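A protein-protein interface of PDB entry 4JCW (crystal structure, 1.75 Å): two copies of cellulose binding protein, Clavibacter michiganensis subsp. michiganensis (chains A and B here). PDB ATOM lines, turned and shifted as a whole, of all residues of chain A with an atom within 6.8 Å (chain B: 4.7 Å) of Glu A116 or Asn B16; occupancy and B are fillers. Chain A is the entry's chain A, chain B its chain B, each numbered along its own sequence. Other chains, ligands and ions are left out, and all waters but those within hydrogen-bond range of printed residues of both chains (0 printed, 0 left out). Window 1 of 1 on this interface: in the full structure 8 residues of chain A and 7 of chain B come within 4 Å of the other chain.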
ATOM      1  N   THR A  17      20.907  12.639  14.326  1.00  0.00           N
ATOM      2  CA  THR A  17      20.454  13.949  14.774  1.00  0.00           C
ATOM      3  C   THR A  17      20.299  14.962  13.634  1.00  0.00           C
ATOM      4  O   THR A  17      20.141  16.148  13.884  1.00  0.00           O
ATOM      5  CB  THR A  17      21.414  14.529  15.833  1.00  0.00           C
ATOM      6  OG1 THR A  17      22.727  14.671  15.272  1.00  0.00           O
ATOM      7  CG2 THR A  17      21.492  13.617  17.035  1.00  0.00           C
ATOM      8  N   ILE A  18      20.334  14.495  12.389  1.00  0.00           N
ATOM      9  CA  ILE A  18      20.288  15.389  11.237  1.00  0.00           C
ATOM     10  C   ILE A  18      18.948  15.295  10.508  1.00  0.00           C
ATOM     11  O   ILE A  18      18.230  16.285  10.344  1.00  0.00           O
ATOM     12  CB  ILE A  18      21.415  15.071  10.217  1.00  0.00           C
ATOM     13  CG1 ILE A  18      22.800  15.138  10.875  1.00  0.00           C
ATOM     14  CG2 ILE A  18      21.326  15.999   9.011  1.00  0.00           C
ATOM     15  CD1 ILE A  18      23.158  16.494  11.455  1.00  0.00           C
ATOM     16  N   ALA A  19      18.615  14.095  10.061  1.00  0.00           N
ATOM     17  CA  ALA A  19      17.473  13.907   9.189  1.00  0.00           C
ATOM     18  C   ALA A  19      17.002  12.467   9.262  1.00  0.00           C
ATOM     19  O   ALA A  19      17.742  11.549   8.901  1.00  0.00           O
ATOM     20  CB  ALA A  19      17.853  14.269   7.758  1.00  0.00           C
ATOM     21  N   ARG A 113      14.467  24.927  13.422  1.00  0.00           N
ATOM     22  CA  ARG A 113      15.819  24.487  13.117  1.00  0.00           C
ATOM     23  C   ARG A 113      16.256  24.998  11.750  1.00  0.00           C
ATOM     24  O   ARG A 113      15.567  24.791  10.764  1.00  0.00           O
ATOM     25  CB  ARG A 113      15.930  22.966  13.158  1.00  0.00           C
ATOM     26  CG  ARG A 113      17.327  22.483  12.829  1.00  0.00           C
ATOM     27  CD  ARG A 113      17.479  21.025  13.135  1.00  0.00           C
ATOM     28  NE  ARG A 113      16.654  20.189  12.277  1.00  0.00           N
ATOM     29  CZ  ARG A 113      16.977  18.934  11.979  1.00  0.00           C
ATOM     30  NH1 ARG A 113      18.090  18.433  12.485  1.00  0.00           N
ATOM     31  NH2 ARG A 113      16.203  18.194  11.192  1.00  0.00           N
ATOM     32  N   VAL A 114      17.400  25.668  11.708  1.00  0.00           N
ATOM     33  CA  VAL A 114      17.975  26.126  10.447  1.00  0.00           C
ATOM     34  C   VAL A 114      18.764  24.968   9.837  1.00  0.00           C
ATOM     35  O   VAL A 114      19.494  24.277  10.548  1.00  0.00           O
ATOM     36  CB  VAL A 114      18.876  27.347  10.689  1.00  0.00           C
ATOM     37  CG1 VAL A 114      19.586  27.752   9.416  1.00  0.00           C
ATOM     38  CG2 VAL A 114      18.041  28.513  11.238  1.00  0.00           C
ATOM     39  N   LYS A 115      18.596  24.745   8.531  1.00  0.00           N
ATOM     40  CA  LYS A 115      19.248  23.626   7.840  1.00  0.00           C
ATOM     41  C   LYS A 115      20.767  23.751   7.835  1.00  0.00           C
ATOM     42  O   LYS A 115      21.307  24.860   7.714  1.00  0.00           O
ATOM     43  CB  LYS A 115      18.765  23.516   6.392  1.00  0.00           C
ATOM     44  CG  LYS A 115      19.060  22.145   5.771  1.00  0.00           C
ATOM     45  CD  LYS A 115      18.485  22.011   4.380  1.00  0.00           C
ATOM     46  CE  LYS A 115      18.696  20.594   3.831  1.00  0.00           C
ATOM     47  NZ  LYS A 115      20.144  20.250   3.673  1.00  0.00           N
ATOM     48  N   GLU A 116      21.449  22.615   7.977  1.00  0.00           N
ATOM     49  CA  GLU A 116      22.893  22.567   7.762  1.00  0.00           C
ATOM     50  C   GLU A 116      23.193  23.203   6.410  1.00  0.00           C
ATOM     51  O   GLU A 116      22.431  23.024   5.452  1.00  0.00           O
ATOM     52  CB  GLU A 116      23.413  21.121   7.791  1.00  0.00           C
ATOM     53  CG  GLU A 116      23.283  20.447   9.141  1.00  0.00           C
ATOM     54  CD  GLU A 116      21.880  19.941   9.424  1.00  0.00           C
ATOM     55  OE1 GLU A 116      21.029  19.968   8.502  1.00  0.00           O
ATOM     56  OE2 GLU A 116      21.626  19.518  10.577  1.00  0.00           O
ATOM     57  N   GLY A 117      24.278  23.970   6.348  1.00  0.00           N
ATOM     58  CA  GLY A 117      24.680  24.621   5.116  1.00  0.00           C
ATOM     59  C   GLY A 117      23.987  25.938   4.803  1.00  0.00           C
ATOM     60  O   GLY A 117      24.300  26.568   3.796  1.00  0.00           O
ATOM     61  N   SER A 118      23.053  26.363   5.650  1.00  0.00           N
ATOM     62  CA  SER A 118      22.326  27.613   5.402  1.00  0.00           C
ATOM     63  C   SER A 118      23.213  28.837   5.594  1.00  0.00           C
ATOM     64  O   SER A 118      24.173  28.805   6.370  1.00  0.00           O
ATOM     65  CB  SER A 118      21.110  27.760   6.331  1.00  0.00           C
ATOM     66  OG  SER A 118      20.074  26.834   6.047  1.00  0.00           O
ATOM     67  N   TRP A 122      21.300  31.494   1.012  1.00  0.00           N
ATOM     68  CA  TRP A 122      20.232  30.517   0.872  1.00  0.00           C
ATOM     69  C   TRP A 122      20.062  29.793   2.193  1.00  0.00           C
ATOM     70  O   TRP A 122      21.044  29.373   2.807  1.00  0.00           O
ATOM     71  CB  TRP A 122      20.575  29.492  -0.216  1.00  0.00           C
ATOM     72  CG  TRP A 122      19.534  28.430  -0.379  1.00  0.00           C
ATOM     73  CD1 TRP A 122      18.473  28.448  -1.236  1.00  0.00           C
ATOM     74  CD2 TRP A 122      19.449  27.191   0.344  1.00  0.00           C
ATOM     75  NE1 TRP A 122      17.733  27.297  -1.094  1.00  0.00           N
ATOM     76  CE2 TRP A 122      18.311  26.508  -0.133  1.00  0.00           C
ATOM     77  CE3 TRP A 122      20.231  26.590   1.340  1.00  0.00           C
ATOM     78  CZ2 TRP A 122      17.936  25.251   0.350  1.00  0.00           C
ATOM     79  CZ3 TRP A 122      19.854  25.337   1.822  1.00  0.00           C
ATOM     80  CH2 TRP A 122      18.712  24.688   1.331  1.00  0.00           C
ATOM     81  N   GLY A 124      17.363  27.040   4.663  1.00  0.00           N
ATOM     82  CA  GLY A 124      16.166  26.262   4.944  1.00  0.00           C
ATOM     83  C   GLY A 124      15.780  26.387   6.407  1.00  0.00           C
ATOM     84  O   GLY A 124      16.653  26.440   7.274  1.00  0.00           O
ATOM     85  N   TYR A 155      11.482  20.964   5.067  1.00  0.00           N
ATOM     86  CA  TYR A 155      12.012  22.299   5.313  1.00  0.00           C
ATOM     87  C   TYR A 155      11.265  23.337   4.491  1.00  0.00           C
ATOM     88  O   TYR A 155      10.503  22.995   3.584  1.00  0.00           O
ATOM     89  CB  TYR A 155      13.505  22.361   4.962  1.00  0.00           C
ATOM     90  CG  TYR A 155      14.406  21.884   6.079  1.00  0.00           C
ATOM     91  CD1 TYR A 155      15.041  22.794   6.917  1.00  0.00           C
ATOM     92  CD2 TYR A 155      14.614  20.522   6.307  1.00  0.00           C
ATOM     93  CE1 TYR A 155      15.867  22.368   7.927  1.00  0.00           C
ATOM     94  CE2 TYR A 155      15.444  20.085   7.330  1.00  0.00           C
ATOM     95  CZ  TYR A 155      16.066  21.017   8.134  1.00  0.00           C
ATOM     96  OH  TYR A 155      16.885  20.619   9.156  1.00  0.00           O
ATOM     97  N   PRO A 188      22.912  27.112  11.820  1.00  0.00           N
ATOM     98  CA  PRO A 188      22.551  25.856  11.151  1.00  0.00           C
ATOM     99  C   PRO A 188      22.666  24.670  12.092  1.00  0.00           C
ATOM    100  O   PRO A 188      23.626  24.597  12.869  1.00  0.00           O
ATOM    101  CB  PRO A 188      23.599  25.742  10.044  1.00  0.00           C
ATOM    102  CG  PRO A 188      23.989  27.143   9.760  1.00  0.00           C
ATOM    103  CD  PRO A 188      23.975  27.829  11.099  1.00  0.00           C
ATOM    104  N   GLY A 189      21.688  23.773  12.034  1.00  0.00           N
ATOM    105  CA  GLY A 189      21.715  22.551  12.815  1.00  0.00           C
ATOM    106  C   GLY A 189      21.144  22.654  14.215  1.00  0.00           C
ATOM    107  O   GLY A 189      20.776  21.642  14.814  1.00  0.00           O
ATOM    108  N   GLU A 190      21.055  23.869  14.745  1.00  0.00           N
ATOM    109  CA  GLU A 190      20.599  24.062  16.119  1.00  0.00           C
ATOM    110  C   GLU A 190      19.071  24.121  16.211  1.00  0.00           C
ATOM    111  O   GLU A 190      18.418  24.744  15.384  1.00  0.00           O
ATOM    112  CB  GLU A 190      21.208  25.347  16.696  1.00  0.00           C
ATOM    113  CG  GLU A 190      20.728  25.688  18.098  1.00  0.00           C
ATOM    114  CD  GLU A 190      21.339  26.971  18.644  1.00  0.00           C
ATOM    115  OE1 GLU A 190      22.271  27.516  18.013  1.00  0.00           O
ATOM    116  OE2 GLU A 190      20.883  27.431  19.713  1.00  0.00           O
ATOM    117  N   GLN B  14      32.005  29.029   6.688  1.00  0.00           N
ATOM    118  CA  GLN B  14      32.766  28.014   7.409  1.00  0.00           C
ATOM    119  C   GLN B  14      32.304  26.600   7.061  1.00  0.00           C
ATOM    120  O   GLN B  14      33.122  25.728   6.767  1.00  0.00           O
ATOM    121  CB  GLN B  14      32.650  28.240   8.918  1.00  0.00           C
ATOM    122  CG  GLN B  14      33.577  27.372   9.753  1.00  0.00           C
ATOM    123  CD  GLN B  14      34.968  27.969   9.907  1.00  0.00           C
ATOM    124  OE1 GLN B  14      35.163  28.939  10.642  1.00  0.00           O
ATOM    125  NE2 GLN B  14      35.943  27.386   9.215  1.00  0.00           N
ATOM    126  N   GLY B  15      30.996  26.368   7.105  1.00  0.00           N
ATOM    127  CA  GLY B  15      30.459  25.087   6.696  1.00  0.00           C
ATOM    128  C   GLY B  15      30.316  24.073   7.811  1.00  0.00           C
ATOM    129  O   GLY B  15      30.498  24.394   8.984  1.00  0.00           O
ATOM    130  N   ASN B  16      29.991  22.841   7.431  1.00  0.00           N
ATOM    131  CA  ASN B  16      29.672  21.785   8.383  1.00  0.00           C
ATOM    132  C   ASN B  16      30.159  20.423   7.869  1.00  0.00           C
ATOM    133  O   ASN B  16      30.796  20.356   6.823  1.00  0.00           O
ATOM    134  CB  ASN B  16      28.160  21.765   8.637  1.00  0.00           C
ATOM    135  CG  ASN B  16      27.358  21.533   7.364  1.00  0.00           C
ATOM    136  OD1 ASN B  16      26.996  20.403   7.057  1.00  0.00           O
ATOM    137  ND2 ASN B  16      27.075  22.607   6.616  1.00  0.00           N
ATOM    138  N   THR B  17      29.852  19.350   8.603  1.00  0.00           N
ATOM    139  CA  THR B  17      30.321  18.008   8.257  1.00  0.00           C
ATOM    140  C   THR B  17      29.267  17.182   7.530  1.00  0.00           C
ATOM    141  O   THR B  17      29.513  16.036   7.173  1.00  0.00           O
ATOM    142  CB  THR B  17      30.752  17.217   9.508  1.00  0.00           C
ATOM    143  OG1 THR B  17      29.606  16.965  10.330  1.00  0.00           O
ATOM    144  CG2 THR B  17      31.780  17.991  10.315  1.00  0.00           C
ATOM    145  N   ILE B  18      28.098  17.765   7.311  1.00  0.00           N
ATOM    146  CA  ILE B  18      26.951  17.044   6.752  1.00  0.00           C
ATOM    147  C   ILE B  18      26.788  17.264   5.251  1.00  0.00           C
ATOM    148  O   ILE B  18      26.831  16.321   4.450  1.00  0.00           O
ATOM    149  CB  ILE B  18      25.648  17.479   7.430  1.00  0.00           C
ATOM    150  CG1 ILE B  18      25.751  17.278   8.942  1.00  0.00           C
ATOM    151  CG2 ILE B  18      24.470  16.722   6.842  1.00  0.00           C
ATOM    152  CD1 ILE B  18      26.115  15.883   9.354  1.00  0.00           C
ATOM    153  N   ALA B  19      26.608  18.517   4.864  1.00  0.00           N
ATOM    154  CA  ALA B  19      26.288  18.820   3.483  1.00  0.00           C
ATOM    155  C   ALA B  19      26.620  20.273   3.206  1.00  0.00           C
ATOM    156  O   ALA B  19      26.077  21.165   3.849  1.00  0.00           O
ATOM    157  CB  ALA B  19      24.818  18.544   3.217  1.00  0.00           C
ATOM    158  N   ASN B  20      27.545  20.498   2.279  1.00  0.00           N
ATOM    159  CA  ASN B  20      27.968  21.832   1.931  1.00  0.00           C
ATOM    160  C   ASN B  20      27.718  22.009   0.447  1.00  0.00           C
ATOM    161  O   ASN B  20      28.231  21.241  -0.374  1.00  0.00           O
ATOM    162  CB  ASN B  20      29.446  22.033   2.268  1.00  0.00           C
ATOM    163  CG  ASN B  20      29.746  21.800   3.733  1.00  0.00           C
ATOM    164  OD1 ASN B  20      29.625  22.712   4.552  1.00  0.00           O
ATOM    165  ND2 ASN B  20      30.142  20.568   4.074  1.00  0.00           N
ATOM    166  N   PRO B  26      31.011  16.759   1.969  1.00  0.00           N
ATOM    167  CA  PRO B  26      31.238  16.486   3.395  1.00  0.00           C
ATOM    168  C   PRO B  26      31.934  17.654   4.084  1.00  0.00           C
ATOM    169  O   PRO B  26      31.895  17.757   5.310  1.00  0.00           O
ATOM    170  CB  PRO B  26      32.188  15.280   3.380  1.00  0.00           C
ATOM    171  CG  PRO B  26      32.127  14.732   1.994  1.00  0.00           C
ATOM    172  CD  PRO B  26      31.831  15.892   1.109  1.00  0.00           C
ATOM    173  N   ALA B  27      32.603  18.498   3.300  1.00  0.00           N
ATOM    174  CA  ALA B  27      33.261  19.674   3.847  1.00  0.00           C
ATOM    175  C   ALA B  27      33.432  20.743   2.789  1.00  0.00           C
ATOM    176  O   ALA B  27      33.508  20.439   1.598  1.00  0.00           O
ATOM    177  CB  ALA B  27      34.621  19.305   4.424  1.00  0.00           C
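Ile A18 touches its own counterpart, Ile B18.
Positions printed for both chains: 17, 18 and 19.
Of the 4 pairs that touch across the chains among the printed residues, 1 has its exchanged pair printed and touching as well.
The backbone NH (N) of Gly A117 lies close to the side-chain amide nitrogen (ND2) of Asn B16, at 3.1 Å.
Among the printed residues, pairs that only touch across the chains: Ile A18 with Ile B18, Glu A116 with Asn B16 and Gly A117 with Ala B19.
Printed residues of chain B within 4 Å of Ile A18: Ile B18 (3.7 Å).
Of chain B, only Asn B16 comes within 4 Å of Glu A116.
Of the printed residues of chain B, Gly A117 touches Asn B16 and Ala B19.
Asn B16 touches two residues of chain A.
Asn B20 touches none of the printed residues of chain A.
The nearest residue of chain B that does not touch Glu A116 is Ile B18 (4.02 Å).
The nearest residue of chain A that does not touch Asn B16 is Ser A118 (5.6 Å).
The nearest printed residue of chain B that does not touch Gly A117 is Asn B20 (5.3 Å).
The guanidinium group of Arg A113 is in hydrogen-bond range of the backbone carbonyl oxygen of Ile A18.
The backbone NH of Ile B18 sits at hydrogen-bond distance from the side-chain amide oxygen of Asn B16 (2.9 Å).
The backbone NH of Ala B19 lies within hydrogen-bond range of the side-chain amide oxygen of Asn B16 (2.9 Å).
ND2 of Asn B20 is in hydrogen-bond range of O of Asn B16 (2.8 Å).
Of the 15 printed residues of chain A, 3 touch a printed residue of chain B.
Printed residues of chain A that touch a printed residue of chain B: Ile A18, Glu A116 and Gly A117.
Of the 9 printed residues of chain B, 3 touch a printed residue of chain A.
Among the printed residues, no Asp or Glu carboxylate lies within 4 Å of a Lys or Arg side-chain nitrogen of the other chain.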
